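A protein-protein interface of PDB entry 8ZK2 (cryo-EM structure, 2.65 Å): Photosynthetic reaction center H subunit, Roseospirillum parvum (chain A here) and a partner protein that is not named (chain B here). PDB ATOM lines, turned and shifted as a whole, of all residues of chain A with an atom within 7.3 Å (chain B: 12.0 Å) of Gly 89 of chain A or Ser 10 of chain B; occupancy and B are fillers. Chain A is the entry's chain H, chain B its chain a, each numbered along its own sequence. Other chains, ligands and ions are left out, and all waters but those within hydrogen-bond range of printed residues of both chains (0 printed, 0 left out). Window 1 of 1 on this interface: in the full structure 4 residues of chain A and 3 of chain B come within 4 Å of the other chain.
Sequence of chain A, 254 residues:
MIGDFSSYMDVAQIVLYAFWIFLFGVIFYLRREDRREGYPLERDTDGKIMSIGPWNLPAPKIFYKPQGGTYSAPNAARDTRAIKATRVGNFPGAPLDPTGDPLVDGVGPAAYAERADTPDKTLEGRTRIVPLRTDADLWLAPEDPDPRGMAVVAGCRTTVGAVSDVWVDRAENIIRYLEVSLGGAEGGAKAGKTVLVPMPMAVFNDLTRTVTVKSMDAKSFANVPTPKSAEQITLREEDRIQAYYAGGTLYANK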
ATOM      1  N   THR A  45      19.158   4.924 -21.748  1.00  0.00           N
ATOM      2  CA  THR A  45      18.831   6.258 -21.262  1.00  0.00           C
ATOM      3  C   THR A  45      17.352   6.599 -21.312  1.00  0.00           C
ATOM      4  O   THR A  45      16.877   7.308 -20.416  1.00  0.00           O
ATOM      5  CB  THR A  45      19.604   7.318 -22.058  1.00  0.00           C
ATOM      6  OG1 THR A  45      19.354   7.142 -23.458  1.00  0.00           O
ATOM      7  CG2 THR A  45      21.086   7.176 -21.809  1.00  0.00           C
ATOM      8  N   THR A  86      17.388   3.805  -8.651  1.00  0.00           N
ATOM      9  CA  THR A  86      17.633   5.093  -9.279  1.00  0.00           C
ATOM     10  C   THR A  86      19.125   5.279  -9.502  1.00  0.00           C
ATOM     11  O   THR A  86      19.959   4.578  -8.925  1.00  0.00           O
ATOM     12  CB  THR A  86      17.081   6.253  -8.437  1.00  0.00           C
ATOM     13  OG1 THR A  86      17.635   6.193  -7.116  1.00  0.00           O
ATOM     14  CG2 THR A  86      15.564   6.193  -8.354  1.00  0.00           C
ATOM     15  N   ARG A  87      19.449   6.236 -10.367  1.00  0.00           N
ATOM     16  CA  ARG A  87      20.819   6.662 -10.599  1.00  0.00           C
ATOM     17  C   ARG A  87      20.828   8.169 -10.802  1.00  0.00           C
ATOM     18  O   ARG A  87      19.828   8.758 -11.221  1.00  0.00           O
ATOM     19  CB  ARG A  87      21.436   5.955 -11.812  1.00  0.00           C
ATOM     20  CG  ARG A  87      20.716   6.233 -13.117  1.00  0.00           C
ATOM     21  CD  ARG A  87      21.319   5.440 -14.259  1.00  0.00           C
ATOM     22  NE  ARG A  87      20.612   5.674 -15.511  1.00  0.00           N
ATOM     23  CZ  ARG A  87      20.942   5.125 -16.671  1.00  0.00           C
ATOM     24  NH1 ARG A  87      21.973   4.304 -16.777  1.00  0.00           N
ATOM     25  NH2 ARG A  87      20.221   5.409 -17.751  1.00  0.00           N
ATOM     26  N   VAL A  88      21.963   8.793 -10.493  1.00  0.00           N
ATOM     27  CA  VAL A  88      22.113  10.238 -10.642  1.00  0.00           C
ATOM     28  C   VAL A  88      22.554  10.502 -12.079  1.00  0.00           C
ATOM     29  O   VAL A  88      23.696  10.229 -12.452  1.00  0.00           O
ATOM     30  CB  VAL A  88      23.100  10.820  -9.628  1.00  0.00           C
ATOM     31  CG1 VAL A  88      23.460  12.251  -9.998  1.00  0.00           C
ATOM     32  CG2 VAL A  88      22.513  10.757  -8.228  1.00  0.00           C
ATOM     33  N   GLY A  89      21.643  11.020 -12.896  1.00  0.00           N
ATOM     34  CA  GLY A  89      21.949  11.282 -14.288  1.00  0.00           C
ATOM     35  C   GLY A  89      21.804  10.048 -15.152  1.00  0.00           C
ATOM     36  O   GLY A  89      22.347   8.989 -14.825  1.00  0.00           O
ATOM     37  N   ASN A  90      21.079  10.170 -16.265  1.00  0.00           N
ATOM     38  CA  ASN A  90      20.842   9.041 -17.163  1.00  0.00           C
ATOM     39  C   ASN A  90      22.023   8.865 -18.123  1.00  0.00           C
ATOM     40  O   ASN A  90      21.924   9.001 -19.343  1.00  0.00           O
ATOM     41  CB  ASN A  90      19.508   9.210 -17.885  1.00  0.00           C
ATOM     42  CG  ASN A  90      19.461  10.437 -18.790  1.00  0.00           C
ATOM     43  OD1 ASN A  90      20.456  11.129 -18.993  1.00  0.00           O
ATOM     44  ND2 ASN A  90      18.285  10.702 -19.346  1.00  0.00           N
ATOM     45  N   PHE A  91      23.159   8.524 -17.541  1.00  0.00           N
ATOM     46  CA  PHE A  91      24.333   8.248 -18.360  1.00  0.00           C
ATOM     47  C   PHE A  91      24.328   6.787 -18.791  1.00  0.00           C
ATOM     48  O   PHE A  91      24.060   5.907 -17.966  1.00  0.00           O
ATOM     49  CB  PHE A  91      25.613   8.550 -17.602  1.00  0.00           C
ATOM     50  CG  PHE A  91      26.842   8.508 -18.460  1.00  0.00           C
ATOM     51  CD1 PHE A  91      27.112   9.531 -19.348  1.00  0.00           C
ATOM     52  CD2 PHE A  91      27.717   7.438 -18.392  1.00  0.00           C
ATOM     53  CE1 PHE A  91      28.234   9.493 -20.145  1.00  0.00           C
ATOM     54  CE2 PHE A  91      28.841   7.398 -19.188  1.00  0.00           C
ATOM     55  CZ  PHE A  91      29.099   8.427 -20.066  1.00  0.00           C
ATOM     56  N   PRO A  92      24.604   6.495 -20.065  1.00  0.00           N
ATOM     57  CA  PRO A  92      24.657   5.098 -20.515  1.00  0.00           C
ATOM     58  C   PRO A  92      25.668   4.270 -19.740  1.00  0.00           C
ATOM     59  O   PRO A  92      26.852   4.618 -19.684  1.00  0.00           O
ATOM     60  CB  PRO A  92      25.058   5.224 -21.988  1.00  0.00           C
ATOM     61  CG  PRO A  92      24.593   6.573 -22.386  1.00  0.00           C
ATOM     62  CD  PRO A  92      24.787   7.439 -21.180  1.00  0.00           C
ATOM     63  N   ALA A  94      25.518   3.651 -16.451  1.00  0.00           N
ATOM     64  CA  ALA A  94      25.542   3.965 -15.032  1.00  0.00           C
ATOM     65  C   ALA A  94      24.672   2.975 -14.261  1.00  0.00           C
ATOM     66  O   ALA A  94      23.487   2.816 -14.567  1.00  0.00           O
ATOM     67  CB  ALA A  94      25.054   5.392 -14.790  1.00  0.00           C
ATOM     68  N   PRO A  95      25.230   2.294 -13.265  1.00  0.00           N
ATOM     69  CA  PRO A  95      24.441   1.322 -12.502  1.00  0.00           C
ATOM     70  C   PRO A  95      23.427   1.998 -11.591  1.00  0.00           C
ATOM     71  O   PRO A  95      23.532   3.183 -11.271  1.00  0.00           O
ATOM     72  CB  PRO A  95      25.502   0.565 -11.698  1.00  0.00           C
ATOM     73  CG  PRO A  95      26.618   1.538 -11.570  1.00  0.00           C
ATOM     74  CD  PRO A  95      26.643   2.300 -12.854  1.00  0.00           C
ATOM     75  N   SER B   9      23.996  17.515 -16.835  1.00  0.00           N
ATOM     76  CA  SER B   9      22.712  17.162 -17.431  1.00  0.00           C
ATOM     77  C   SER B   9      22.574  15.650 -17.553  1.00  0.00           C
ATOM     78  O   SER B   9      21.996  15.000 -16.683  1.00  0.00           O
ATOM     79  CB  SER B   9      22.556  17.819 -18.802  1.00  0.00           C
ATOM     80  OG  SER B   9      23.407  17.215 -19.760  1.00  0.00           O
ATOM     81  N   SER B  10      23.106  15.097 -18.645  1.00  0.00           N
ATOM     82  CA  SER B  10      23.098  13.648 -18.821  1.00  0.00           C
ATOM     83  C   SER B  10      23.946  12.957 -17.763  1.00  0.00           C
ATOM     84  O   SER B  10      23.551  11.920 -17.220  1.00  0.00           O
ATOM     85  CB  SER B  10      23.592  13.287 -20.220  1.00  0.00           C
ATOM     86  OG  SER B  10      23.717  11.884 -20.367  1.00  0.00           O
ATOM     87  N   THR B  11      25.116  13.518 -17.456  1.00  0.00           N
ATOM     88  CA  THR B  11      26.010  12.911 -16.481  1.00  0.00           C
ATOM     89  C   THR B  11      25.618  13.239 -15.048  1.00  0.00           C
ATOM     90  O   THR B  11      26.229  12.709 -14.113  1.00  0.00           O
ATOM     91  CB  THR B  11      27.448  13.360 -16.742  1.00  0.00           C
ATOM     92  OG1 THR B  11      27.567  14.759 -16.463  1.00  0.00           O
ATOM     93  CG2 THR B  11      27.817  13.116 -18.187  1.00  0.00           C
ATOM     94  N   GLY B  12      24.620  14.095 -14.853  1.00  0.00           N
ATOM     95  CA  GLY B  12      24.217  14.511 -13.529  1.00  0.00           C
ATOM     96  C   GLY B  12      24.947  15.718 -12.992  1.00  0.00           C
ATOM     97  O   GLY B  12      24.619  16.181 -11.893  1.00  0.00           O
ATOM     98  N   LEU B  13      25.923  16.242 -13.725  1.00  0.00           N
ATOM     99  CA  LEU B  13      26.655  17.425 -13.305  1.00  0.00           C
ATOM    100  C   LEU B  13      25.905  18.691 -13.701  1.00  0.00           C
ATOM    101  O   LEU B  13      25.130  18.715 -14.660  1.00  0.00           O
ATOM    102  CB  LEU B  13      28.058  17.446 -13.918  1.00  0.00           C
ATOM    103  CG  LEU B  13      29.169  16.657 -13.226  1.00  0.00           C
ATOM    104  CD1 LEU B  13      29.053  15.170 -13.518  1.00  0.00           C
ATOM    105  CD2 LEU B  13      30.531  17.185 -13.642  1.00  0.00           C
ATOM    106  N   THR B  14      26.143  19.748 -12.936  1.00  0.00           N
ATOM    107  CA  THR B  14      25.654  21.078 -13.252  1.00  0.00           C
ATOM    108  C   THR B  14      26.701  21.793 -14.098  1.00  0.00           C
ATOM    109  O   THR B  14      27.896  21.504 -14.000  1.00  0.00           O
ATOM    110  CB  THR B  14      25.368  21.871 -11.973  1.00  0.00           C
ATOM    111  OG1 THR B  14      24.570  21.075 -11.090  1.00  0.00           O
ATOM    112  CG2 THR B  14      24.616  23.155 -12.282  1.00  0.00           C
ATOM    113  N   GLU B  15      26.244  22.717 -14.947  1.00  0.00           N
ATOM    114  CA  GLU B  15      27.178  23.452 -15.795  1.00  0.00           C
ATOM    115  C   GLU B  15      28.221  24.192 -14.968  1.00  0.00           C
ATOM    116  O   GLU B  15      29.359  24.368 -15.416  1.00  0.00           O
ATOM    117  CB  GLU B  15      26.423  24.427 -16.699  1.00  0.00           C
ATOM    118  CG  GLU B  15      27.323  25.173 -17.670  1.00  0.00           C
ATOM    119  CD  GLU B  15      26.561  26.096 -18.593  1.00  0.00           C
ATOM    120  OE1 GLU B  15      25.321  26.178 -18.469  1.00  0.00           O
ATOM    121  OE2 GLU B  15      27.205  26.742 -19.445  1.00  0.00           O
ATOM    122  N   ALA B  16      27.856  24.631 -13.761  1.00  0.00           N
ATOM    123  CA  ALA B  16      28.840  25.211 -12.854  1.00  0.00           C
ATOM    124  C   ALA B  16      29.881  24.183 -12.428  1.00  0.00           C
ATOM    125  O   ALA B  16      31.080  24.481 -12.416  1.00  0.00           O
ATOM    126  CB  ALA B  16      28.144  25.804 -11.630  1.00  0.00           C
ATOM    127  N   GLU B  17      29.443  22.972 -12.069  1.00  0.00           N
ATOM    128  CA  GLU B  17      30.381  21.902 -11.752  1.00  0.00           C
ATOM    129  C   GLU B  17      31.216  21.499 -12.957  1.00  0.00           C
ATOM    130  O   GLU B  17      32.427  21.285 -12.817  1.00  0.00           O
ATOM    131  CB  GLU B  17      29.639  20.675 -11.226  1.00  0.00           C
ATOM    132  CG  GLU B  17      28.666  20.951 -10.100  1.00  0.00           C
ATOM    133  CD  GLU B  17      27.974  19.692  -9.621  1.00  0.00           C
ATOM    134  OE1 GLU B  17      28.655  18.824  -9.036  1.00  0.00           O
ATOM    135  OE2 GLU B  17      26.750  19.565  -9.834  1.00  0.00           O
ATOM    136  N   ALA B  18      30.593  21.390 -14.131  1.00  0.00           N
ATOM    137  CA  ALA B  18      31.322  21.047 -15.343  1.00  0.00           C
ATOM    138  C   ALA B  18      32.362  22.097 -15.696  1.00  0.00           C
ATOM    139  O   ALA B  18      33.449  21.746 -16.155  1.00  0.00           O
ATOM    140  CB  ALA B  18      30.352  20.857 -16.509  1.00  0.00           C
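The backbone carbonyl oxygen (O) of Ser 10 of chain B is in hydrogen-bond range of the backbone NH (N) of Asn 90 of chain A. N of Phe 91 of chain A sits at hydrogen-bond distance from O of Ser 10 of chain B, 3.4 Å away.
The guanidinium group (NH1) of Arg 87 of chain A is in hydrogen-bond range of the backbone carbonyl oxygen (O) of Phe 91 of chain A.
Among the printed residues, pairs that only touch across the chains: Val 88 of chain A with Thr 11 of chain B, Gly 89 of chain A with Ser 10 of chain B, Gly 89 of chain A with Gly 12 of chain B and Phe 91 of chain A with Thr 11 of chain B.
Thr 86 of chain A touches none of the printed residues of chain B. No residue of chain B comes within 4 Å of Arg 87 of chain A. Val 88 of chain A touches just one residue of chain B: Thr 11 (3.9 Å). Of chain B, only Ser 10 and Gly 12 come within 4 Å of Gly 89 of chain A. Asn 90 of chain A touches one residue of chain B. Phe 91 of chain A touches just these residues of chain B: Ser 10 and Thr 11. No residue of chain B comes within 4 Å of Pro 92 of chain A. Ala 94 of chain A touches none of the printed residues of chain B. No residue of chain A comes within 4 Å of Ser 9 of chain B. Ser 10 of chain B touches just these residues of chain A: Gly 89 (3.3 Å), Asn 90 (3.2 Å) and Phe 91 (3.4 Å). Of the printed residues of chain A, Thr 11 of chain B touches Val 88 (3.9 Å) and Phe 91 (3.8 Å). Printed residues of chain A within 4 Å of Gly 12 of chain B: Gly 89 (3.9 Å). The nearest residue of chain B that does not touch Gly 89 of chain A is Thr 11 of chain B (4.2 Å). The nearest residue of chain A that does not touch Ser 10 of chain B is Pro 92 of chain A (4.6 Å).
Of the 10 printed residues of chain A, 4 touch a printed residue of chain B. Printed residues of chain A that touch a printed residue of chain B: Val 88, Gly 89, Asn 90 and Phe 91. Hydrophobic or aromatic side chains of chain A that line the printed part of chain B: Phe 91. Along chain A the printed residues that touch a printed residue of chain B span positions 88 to 91. Of the 10 printed residues of chain B, 3 touch a printed residue of chain A. Among the printed residues, no Asp or Glu carboxylate lies within 4 Å of a Lys or Arg side-chain nitrogen of the other chain.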
